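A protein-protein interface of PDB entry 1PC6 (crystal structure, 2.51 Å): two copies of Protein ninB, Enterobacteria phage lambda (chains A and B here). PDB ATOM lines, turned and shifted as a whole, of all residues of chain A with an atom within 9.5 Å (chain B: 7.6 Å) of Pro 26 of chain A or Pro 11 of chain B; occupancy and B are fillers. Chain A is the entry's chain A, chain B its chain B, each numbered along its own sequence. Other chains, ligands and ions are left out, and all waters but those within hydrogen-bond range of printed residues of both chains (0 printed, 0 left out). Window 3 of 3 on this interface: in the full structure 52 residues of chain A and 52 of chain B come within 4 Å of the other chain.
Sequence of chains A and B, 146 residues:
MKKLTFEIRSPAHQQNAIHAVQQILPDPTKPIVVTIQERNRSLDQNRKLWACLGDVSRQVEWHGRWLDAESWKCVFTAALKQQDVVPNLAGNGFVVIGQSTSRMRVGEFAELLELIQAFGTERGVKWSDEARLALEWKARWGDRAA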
ATOM      1  N   ALA A  20     -12.164  -5.788  11.154  1.00  0.00           N
ATOM      2  CA  ALA A  20     -13.416  -5.607  10.452  1.00  0.00           C
ATOM      3  C   ALA A  20     -14.147  -6.924  10.448  1.00  0.00           C
ATOM      4  O   ALA A  20     -15.332  -6.979  10.747  1.00  0.00           O
ATOM      5  CB  ALA A  20     -13.161  -5.165   9.039  1.00  0.00           C
ATOM      6  N   VAL A  21     -13.441  -7.994  10.113  1.00  0.00           N
ATOM      7  CA  VAL A  21     -14.075  -9.305  10.081  1.00  0.00           C
ATOM      8  C   VAL A  21     -14.593  -9.695  11.459  1.00  0.00           C
ATOM      9  O   VAL A  21     -15.594 -10.402  11.573  1.00  0.00           O
ATOM     10  CB  VAL A  21     -13.106 -10.392   9.599  1.00  0.00           C
ATOM     11  CG1 VAL A  21     -13.822 -11.735   9.595  1.00  0.00           C
ATOM     12  CG2 VAL A  21     -12.577 -10.047   8.205  1.00  0.00           C
ATOM     13  N   GLN A  22     -13.901  -9.234  12.501  1.00  0.00           N
ATOM     14  CA  GLN A  22     -14.294  -9.526  13.882  1.00  0.00           C
ATOM     15  C   GLN A  22     -15.539  -8.721  14.236  1.00  0.00           C
ATOM     16  O   GLN A  22     -16.420  -9.207  14.950  1.00  0.00           O
ATOM     17  CB  GLN A  22     -13.146  -9.194  14.863  1.00  0.00           C
ATOM     18  N   GLN A  23     -15.611  -7.493  13.724  1.00  0.00           N
ATOM     19  CA  GLN A  23     -16.743  -6.610  13.988  1.00  0.00           C
ATOM     20  C   GLN A  23     -18.031  -7.135  13.346  1.00  0.00           C
ATOM     21  O   GLN A  23     -19.070  -6.475  13.380  1.00  0.00           O
ATOM     22  CB  GLN A  23     -16.432  -5.191  13.484  1.00  0.00           C
ATOM     23  N   ILE A  24     -17.965  -8.336  12.778  1.00  0.00           N
ATOM     24  CA  ILE A  24     -19.126  -8.934  12.125  1.00  0.00           C
ATOM     25  C   ILE A  24     -20.071  -9.621  13.111  1.00  0.00           C
ATOM     26  O   ILE A  24     -19.646 -10.209  14.108  1.00  0.00           O
ATOM     27  CB  ILE A  24     -18.682  -9.955  11.029  1.00  0.00           C
ATOM     28  CG1 ILE A  24     -17.890  -9.234   9.933  1.00  0.00           C
ATOM     29  CG2 ILE A  24     -19.893 -10.632  10.417  1.00  0.00           C
ATOM     30  CD1 ILE A  24     -17.278 -10.147   8.899  1.00  0.00           C
ATOM     31  N   LEU A  25     -21.363  -9.522  12.828  1.00  0.00           N
ATOM     32  CA  LEU A  25     -22.386 -10.142  13.655  1.00  0.00           C
ATOM     33  C   LEU A  25     -22.869 -11.392  12.937  1.00  0.00           C
ATOM     34  O   LEU A  25     -23.600 -11.301  11.952  1.00  0.00           O
ATOM     35  CB  LEU A  25     -23.554  -9.175  13.853  1.00  0.00           C
ATOM     36  CG  LEU A  25     -24.903  -9.708  14.352  1.00  0.00           C
ATOM     37  CD1 LEU A  25     -24.781 -10.311  15.738  1.00  0.00           C
ATOM     38  CD2 LEU A  25     -25.901  -8.561  14.363  1.00  0.00           C
ATOM     39  N   PRO A  26     -22.450 -12.577  13.403  1.00  0.00           N
ATOM     40  CA  PRO A  26     -22.906 -13.791  12.723  1.00  0.00           C
ATOM     41  C   PRO A  26     -24.425 -13.801  12.584  1.00  0.00           C
ATOM     42  O   PRO A  26     -25.138 -13.147  13.346  1.00  0.00           O
ATOM     43  CB  PRO A  26     -22.373 -14.907  13.614  1.00  0.00           C
ATOM     44  CG  PRO A  26     -21.081 -14.328  14.107  1.00  0.00           C
ATOM     45  CD  PRO A  26     -21.465 -12.896  14.450  1.00  0.00           C
ATOM     46  N   ASP A  27     -24.916 -14.546  11.605  1.00  0.00           N
ATOM     47  CA  ASP A  27     -26.341 -14.604  11.344  1.00  0.00           C
ATOM     48  C   ASP A  27     -26.611 -15.803  10.434  1.00  0.00           C
ATOM     49  O   ASP A  27     -26.239 -15.805   9.262  1.00  0.00           O
ATOM     50  CB  ASP A  27     -26.766 -13.288  10.667  1.00  0.00           C
ATOM     51  CG  ASP A  27     -28.256 -13.219  10.370  1.00  0.00           C
ATOM     52  OD1 ASP A  27     -28.688 -12.230   9.732  1.00  0.00           O
ATOM     53  OD2 ASP A  27     -28.994 -14.143  10.773  1.00  0.00           O
ATOM     54  N   PRO A  28     -27.248 -16.853  10.971  1.00  0.00           N
ATOM     55  CA  PRO A  28     -27.545 -18.042  10.161  1.00  0.00           C
ATOM     56  C   PRO A  28     -28.413 -17.669   8.958  1.00  0.00           C
ATOM     57  O   PRO A  28     -28.067 -17.950   7.808  1.00  0.00           O
ATOM     58  CB  PRO A  28     -28.298 -18.948  11.137  1.00  0.00           C
ATOM     59  CG  PRO A  28     -27.773 -18.535  12.476  1.00  0.00           C
ATOM     60  CD  PRO A  28     -27.714 -17.030  12.357  1.00  0.00           C
ATOM     61  N   THR A  29     -29.539 -17.025   9.253  1.00  0.00           N
ATOM     62  CA  THR A  29     -30.509 -16.596   8.248  1.00  0.00           C
ATOM     63  C   THR A  29     -29.899 -15.821   7.072  1.00  0.00           C
ATOM     64  O   THR A  29     -29.802 -16.344   5.963  1.00  0.00           O
ATOM     65  CB  THR A  29     -31.644 -15.743   8.913  1.00  0.00           C
ATOM     66  OG1 THR A  29     -31.111 -14.503   9.403  1.00  0.00           O
ATOM     67  CG2 THR A  29     -32.276 -16.515  10.084  1.00  0.00           C
ATOM     68  N   LYS A  30     -29.500 -14.577   7.310  1.00  0.00           N
ATOM     69  CA  LYS A  30     -28.906 -13.762   6.258  1.00  0.00           C
ATOM     70  C   LYS A  30     -27.421 -13.567   6.548  1.00  0.00           C
ATOM     71  O   LYS A  30     -27.012 -12.498   7.002  1.00  0.00           O
ATOM     72  CB  LYS A  30     -29.612 -12.404   6.180  1.00  0.00           C
ATOM     73  N   PRO A  31     -26.594 -14.605   6.295  1.00  0.00           N
ATOM     74  CA  PRO A  31     -25.149 -14.526   6.540  1.00  0.00           C
ATOM     75  C   PRO A  31     -24.425 -13.633   5.541  1.00  0.00           C
ATOM     76  O   PRO A  31     -24.903 -13.432   4.414  1.00  0.00           O
ATOM     77  CB  PRO A  31     -24.703 -15.983   6.442  1.00  0.00           C
ATOM     78  CG  PRO A  31     -25.614 -16.529   5.406  1.00  0.00           C
ATOM     79  CD  PRO A  31     -26.959 -15.945   5.801  1.00  0.00           C
ATOM     80  N   ILE A  32     -23.286 -13.083   5.968  1.00  0.00           N
ATOM     81  CA  ILE A  32     -22.484 -12.226   5.101  1.00  0.00           C
ATOM     82  C   ILE A  32     -21.208 -12.959   4.691  1.00  0.00           C
ATOM     83  O   ILE A  32     -20.699 -13.820   5.419  1.00  0.00           O
ATOM     84  CB  ILE A  32     -22.132 -10.853   5.764  1.00  0.00           C
ATOM     85  CG1 ILE A  32     -21.098 -11.024   6.866  1.00  0.00           C
ATOM     86  CG2 ILE A  32     -23.388 -10.214   6.331  1.00  0.00           C
ATOM     87  CD1 ILE A  32     -20.587  -9.704   7.380  1.00  0.00           C
ATOM     88  N   ILE B   8     -20.085 -16.585   7.134  1.00  0.00           N
ATOM     89  CA  ILE B   8     -20.044 -16.372   8.573  1.00  0.00           C
ATOM     90  C   ILE B   8     -21.416 -16.484   9.239  1.00  0.00           C
ATOM     91  O   ILE B   8     -22.068 -15.470   9.495  1.00  0.00           O
ATOM     92  CB  ILE B   8     -19.427 -14.993   8.885  1.00  0.00           C
ATOM     93  CG1 ILE B   8     -18.042 -14.904   8.241  1.00  0.00           C
ATOM     94  CG2 ILE B   8     -19.342 -14.778  10.387  1.00  0.00           C
ATOM     95  CD1 ILE B   8     -17.312 -13.635   8.546  1.00  0.00           C
ATOM     96  N   ARG B   9     -21.849 -17.713   9.528  1.00  0.00           N
ATOM     97  CA  ARG B   9     -23.150 -17.940  10.162  1.00  0.00           C
ATOM     98  C   ARG B   9     -23.019 -18.101  11.673  1.00  0.00           C
ATOM     99  O   ARG B   9     -23.863 -17.618  12.429  1.00  0.00           O
ATOM    100  CB  ARG B   9     -23.829 -19.177   9.565  1.00  0.00           C
ATOM    101  CG  ARG B   9     -23.868 -19.168   8.046  1.00  0.00           C
ATOM    102  CD  ARG B   9     -24.792 -20.238   7.493  1.00  0.00           C
ATOM    103  NE  ARG B   9     -24.206 -20.933   6.349  1.00  0.00           N
ATOM    104  CZ  ARG B   9     -23.212 -21.811   6.443  1.00  0.00           C
ATOM    105  NH1 ARG B   9     -22.693 -22.107   7.630  1.00  0.00           N
ATOM    106  NH2 ARG B   9     -22.733 -22.397   5.353  1.00  0.00           N
ATOM    107  N   SER B  10     -21.958 -18.777  12.107  1.00  0.00           N
ATOM    108  CA  SER B  10     -21.710 -19.000  13.531  1.00  0.00           C
ATOM    109  C   SER B  10     -20.467 -18.242  13.963  1.00  0.00           C
ATOM    110  O   SER B  10     -19.642 -17.874  13.132  1.00  0.00           O
ATOM    111  CB  SER B  10     -21.486 -20.487  13.815  1.00  0.00           C
ATOM    112  OG  SER B  10     -20.248 -20.924  13.277  1.00  0.00           O
ATOM    113  N   PRO B  11     -20.320 -17.990  15.271  1.00  0.00           N
ATOM    114  CA  PRO B  11     -19.143 -17.270  15.762  1.00  0.00           C
ATOM    115  C   PRO B  11     -17.859 -18.076  15.528  1.00  0.00           C
ATOM    116  O   PRO B  11     -16.768 -17.510  15.417  1.00  0.00           O
ATOM    117  CB  PRO B  11     -19.460 -17.072  17.241  1.00  0.00           C
ATOM    118  CG  PRO B  11     -20.946 -16.905  17.229  1.00  0.00           C
ATOM    119  CD  PRO B  11     -21.364 -18.035  16.310  1.00  0.00           C
ATOM    120  N   ALA B  12     -17.992 -19.397  15.458  1.00  0.00           N
ATOM    121  CA  ALA B  12     -16.840 -20.251  15.210  1.00  0.00           C
ATOM    122  C   ALA B  12     -16.422 -20.001  13.768  1.00  0.00           C
ATOM    123  O   ALA B  12     -15.236 -19.956  13.448  1.00  0.00           O
ATOM    124  CB  ALA B  12     -17.210 -21.710  15.403  1.00  0.00           C
ATOM    125  N   HIS B  13     -17.420 -19.838  12.904  1.00  0.00           N
ATOM    126  CA  HIS B  13     -17.193 -19.562  11.493  1.00  0.00           C
ATOM    127  C   HIS B  13     -16.280 -18.359  11.286  1.00  0.00           C
ATOM    128  O   HIS B  13     -15.300 -18.443  10.552  1.00  0.00           O
ATOM    129  CB  HIS B  13     -18.519 -19.284  10.794  1.00  0.00           C
ATOM    130  CG  HIS B  13     -19.211 -20.508  10.295  1.00  0.00           C
ATOM    131  ND1 HIS B  13     -18.552 -21.502   9.605  1.00  0.00           N
ATOM    132  CD2 HIS B  13     -20.516 -20.864  10.317  1.00  0.00           C
ATOM    133  CE1 HIS B  13     -19.423 -22.417   9.219  1.00  0.00           C
ATOM    134  NE2 HIS B  13     -20.622 -22.054   9.637  1.00  0.00           N
ATOM    135  N   GLN B  14     -16.613 -17.237  11.926  1.00  0.00           N
ATOM    136  CA  GLN B  14     -15.824 -16.020  11.791  1.00  0.00           C
ATOM    137  C   GLN B  14     -14.526 -16.100  12.568  1.00  0.00           C
ATOM    138  O   GLN B  14     -13.626 -15.282  12.373  1.00  0.00           O
ATOM    139  CB  GLN B  14     -16.611 -14.788  12.249  1.00  0.00           C
ATOM    140  CG  GLN B  14     -16.771 -14.631  13.743  1.00  0.00           C
ATOM    141  CD  GLN B  14     -17.091 -13.199  14.139  1.00  0.00           C
ATOM    142  OE1 GLN B  14     -17.434 -12.919  15.285  1.00  0.00           O
ATOM    143  NE2 GLN B  14     -16.970 -12.283  13.189  1.00  0.00           N
ATOM    144  N   GLN B  15     -14.429 -17.078  13.460  1.00  0.00           N
ATOM    145  CA  GLN B  15     -13.206 -17.243  14.234  1.00  0.00           C
ATOM    146  C   GLN B  15     -12.178 -17.820  13.259  1.00  0.00           C
ATOM    147  O   GLN B  15     -10.991 -17.501  13.324  1.00  0.00           O
ATOM    148  CB  GLN B  15     -13.437 -18.202  15.411  1.00  0.00           C
ATOM    149  CG  GLN B  15     -12.393 -18.112  16.537  1.00  0.00           C
ATOM    150  CD  GLN B  15     -12.570 -16.881  17.421  1.00  0.00           C
ATOM    151  OE1 GLN B  15     -12.387 -15.746  16.975  1.00  0.00           O
ATOM    152  NE2 GLN B  15     -12.931 -17.107  18.684  1.00  0.00           N
ATOM    153  N   ASN B  16     -12.660 -18.667  12.351  1.00  0.00           N
ATOM    154  CA  ASN B  16     -11.820 -19.289  11.335  1.00  0.00           C
ATOM    155  C   ASN B  16     -11.500 -18.275  10.250  1.00  0.00           C
ATOM    156  O   ASN B  16     -10.429 -18.318   9.645  1.00  0.00           O
ATOM    157  CB  ASN B  16     -12.533 -20.488  10.707  1.00  0.00           C
ATOM    158  CG  ASN B  16     -11.921 -20.899   9.368  1.00  0.00           C
ATOM    159  OD1 ASN B  16     -10.714 -21.121   9.269  1.00  0.00           O
ATOM    160  ND2 ASN B  16     -12.756 -21.004   8.335  1.00  0.00           N
ATOM    161  N   ALA B  17     -12.445 -17.375   9.991  1.00  0.00           N
ATOM    162  CA  ALA B  17     -12.247 -16.340   8.985  1.00  0.00           C
ATOM    163  C   ALA B  17     -11.087 -15.487   9.465  1.00  0.00           C
ATOM    164  O   ALA B  17     -10.220 -15.099   8.684  1.00  0.00           O
ATOM    165  CB  ALA B  17     -13.500 -15.491   8.843  1.00  0.00           C
ATOM    166  N   ILE B  18     -11.075 -15.217  10.769  1.00  0.00           N
ATOM    167  CA  ILE B  18     -10.027 -14.416  11.384  1.00  0.00           C
ATOM    168  C   ILE B  18      -8.669 -15.112  11.312  1.00  0.00           C
ATOM    169  O   ILE B  18      -7.630 -14.459  11.341  1.00  0.00           O
ATOM    170  CB  ILE B  18     -10.378 -14.091  12.848  1.00  0.00           C
ATOM    171  CG1 ILE B  18     -11.579 -13.131  12.881  1.00  0.00           C
ATOM    172  CG2 ILE B  18      -9.159 -13.512  13.562  1.00  0.00           C
ATOM    173  CD1 ILE B  18     -11.945 -12.610  14.267  1.00  0.00           C
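The backbone carbonyl oxygen (O) of Val 21 of chain A is in hydrogen-bond range of the side-chain amide nitrogen (NE2) of Gln 14 of chain B (2.8 Å). N of Asp 27 of chain A is in hydrogen-bond range of O of Arg 9 of chain B (3.4 Å). The backbone carbonyl oxygen (O) of Ile 32 of chain A lies within hydrogen-bond range of the backbone NH (N) of Ile 8 of chain B.
OD2 of Asp 27 of chain A lies within hydrogen-bond range of OG1 of Thr 29 of chain A, at 2.5 Å. The backbone NH of Lys 30 of chain A sits at hydrogen-bond distance from the side-chain carboxylate of Asp 27 of chain A (3.5 Å). A ring nitrogen (NE2) of His 13 of chain B sits at hydrogen-bond distance from the guanidinium group (NH1) of Arg 9 of chain B (2.9 Å). The side-chain hydroxyl (OG) of Ser 10 of chain B lies close to the backbone NH (N) of Ala 12 of chain B, 3.5 Å away. OG of Ser 10 of chain B lies close to N of His 13 of chain B (3.1 Å).
CB of Ala 17 of chain B touches CG1 of Val 21 of chain A (3.8 Å). Gln 22 of chain A touches Gln 14 of chain B. Gln 22 of chain A touches Ile 18 of chain B. Pro 26 of chain A touches Ile 8 of chain B. Arg 9 of chain B touches Pro 26 of chain A. Pro 26 of chain A touches Ser 10 of chain B. Pro 26 of chain A touches Pro 11 of chain B (CG to CA, 3.9 Å). Ile 8 of chain B touches Asp 27 of chain A (O to N, 3.7 Å). Pro 28 of chain A touches Arg 9 of chain B (N to O, 3.8 Å). Pro 31 of chain A touches Arg 9 of chain B.
Pro 26 of chain A touches just these residues of chain B: Ile 8, Arg 9, Ser 10 and Pro 11. Pro 11 of chain B touches one residue of chain A. Of chain A, only Pro 26 (3.9 Å) comes within 4 Å of Ser 10 of chain B. Of chain A, only Val 21 (2.8 Å), Gln 22 (3.6 Å) and Ile 24 (3.5 Å) come within 4 Å of Gln 14 of chain B. Of the printed residues of chain B, Gln 22 of chain A touches Gln 14 and Ile 18. Printed residues of chain A within 4 Å of Ile 8 of chain B: Ile 24 (3.5 Å), Pro 26 (3.7 Å), Asp 27 (3.7 Å) and Ile 32 (3.3 Å). Printed residues of chain B within 4 Å of Pro 28 of chain A: Arg 9 (3.8 Å). The nearest residue of chain A that does not touch Pro 11 of chain B is Asp 27 of chain A (6.8 Å).
Along chain A the printed residues that touch a printed residue of chain B span positions 21 to 32. Of the 11 printed residues of chain B, 7 touch a printed residue of chain A. Hydrophobic or aromatic side chains of chain B that line the printed part of chain A: Ile 8, Ala 17 and Ile 18.
No position is printed for both chains. Of the 15 pairs that touch across the chains among the printed residues, none has its exchanged pair printed and touching as well.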
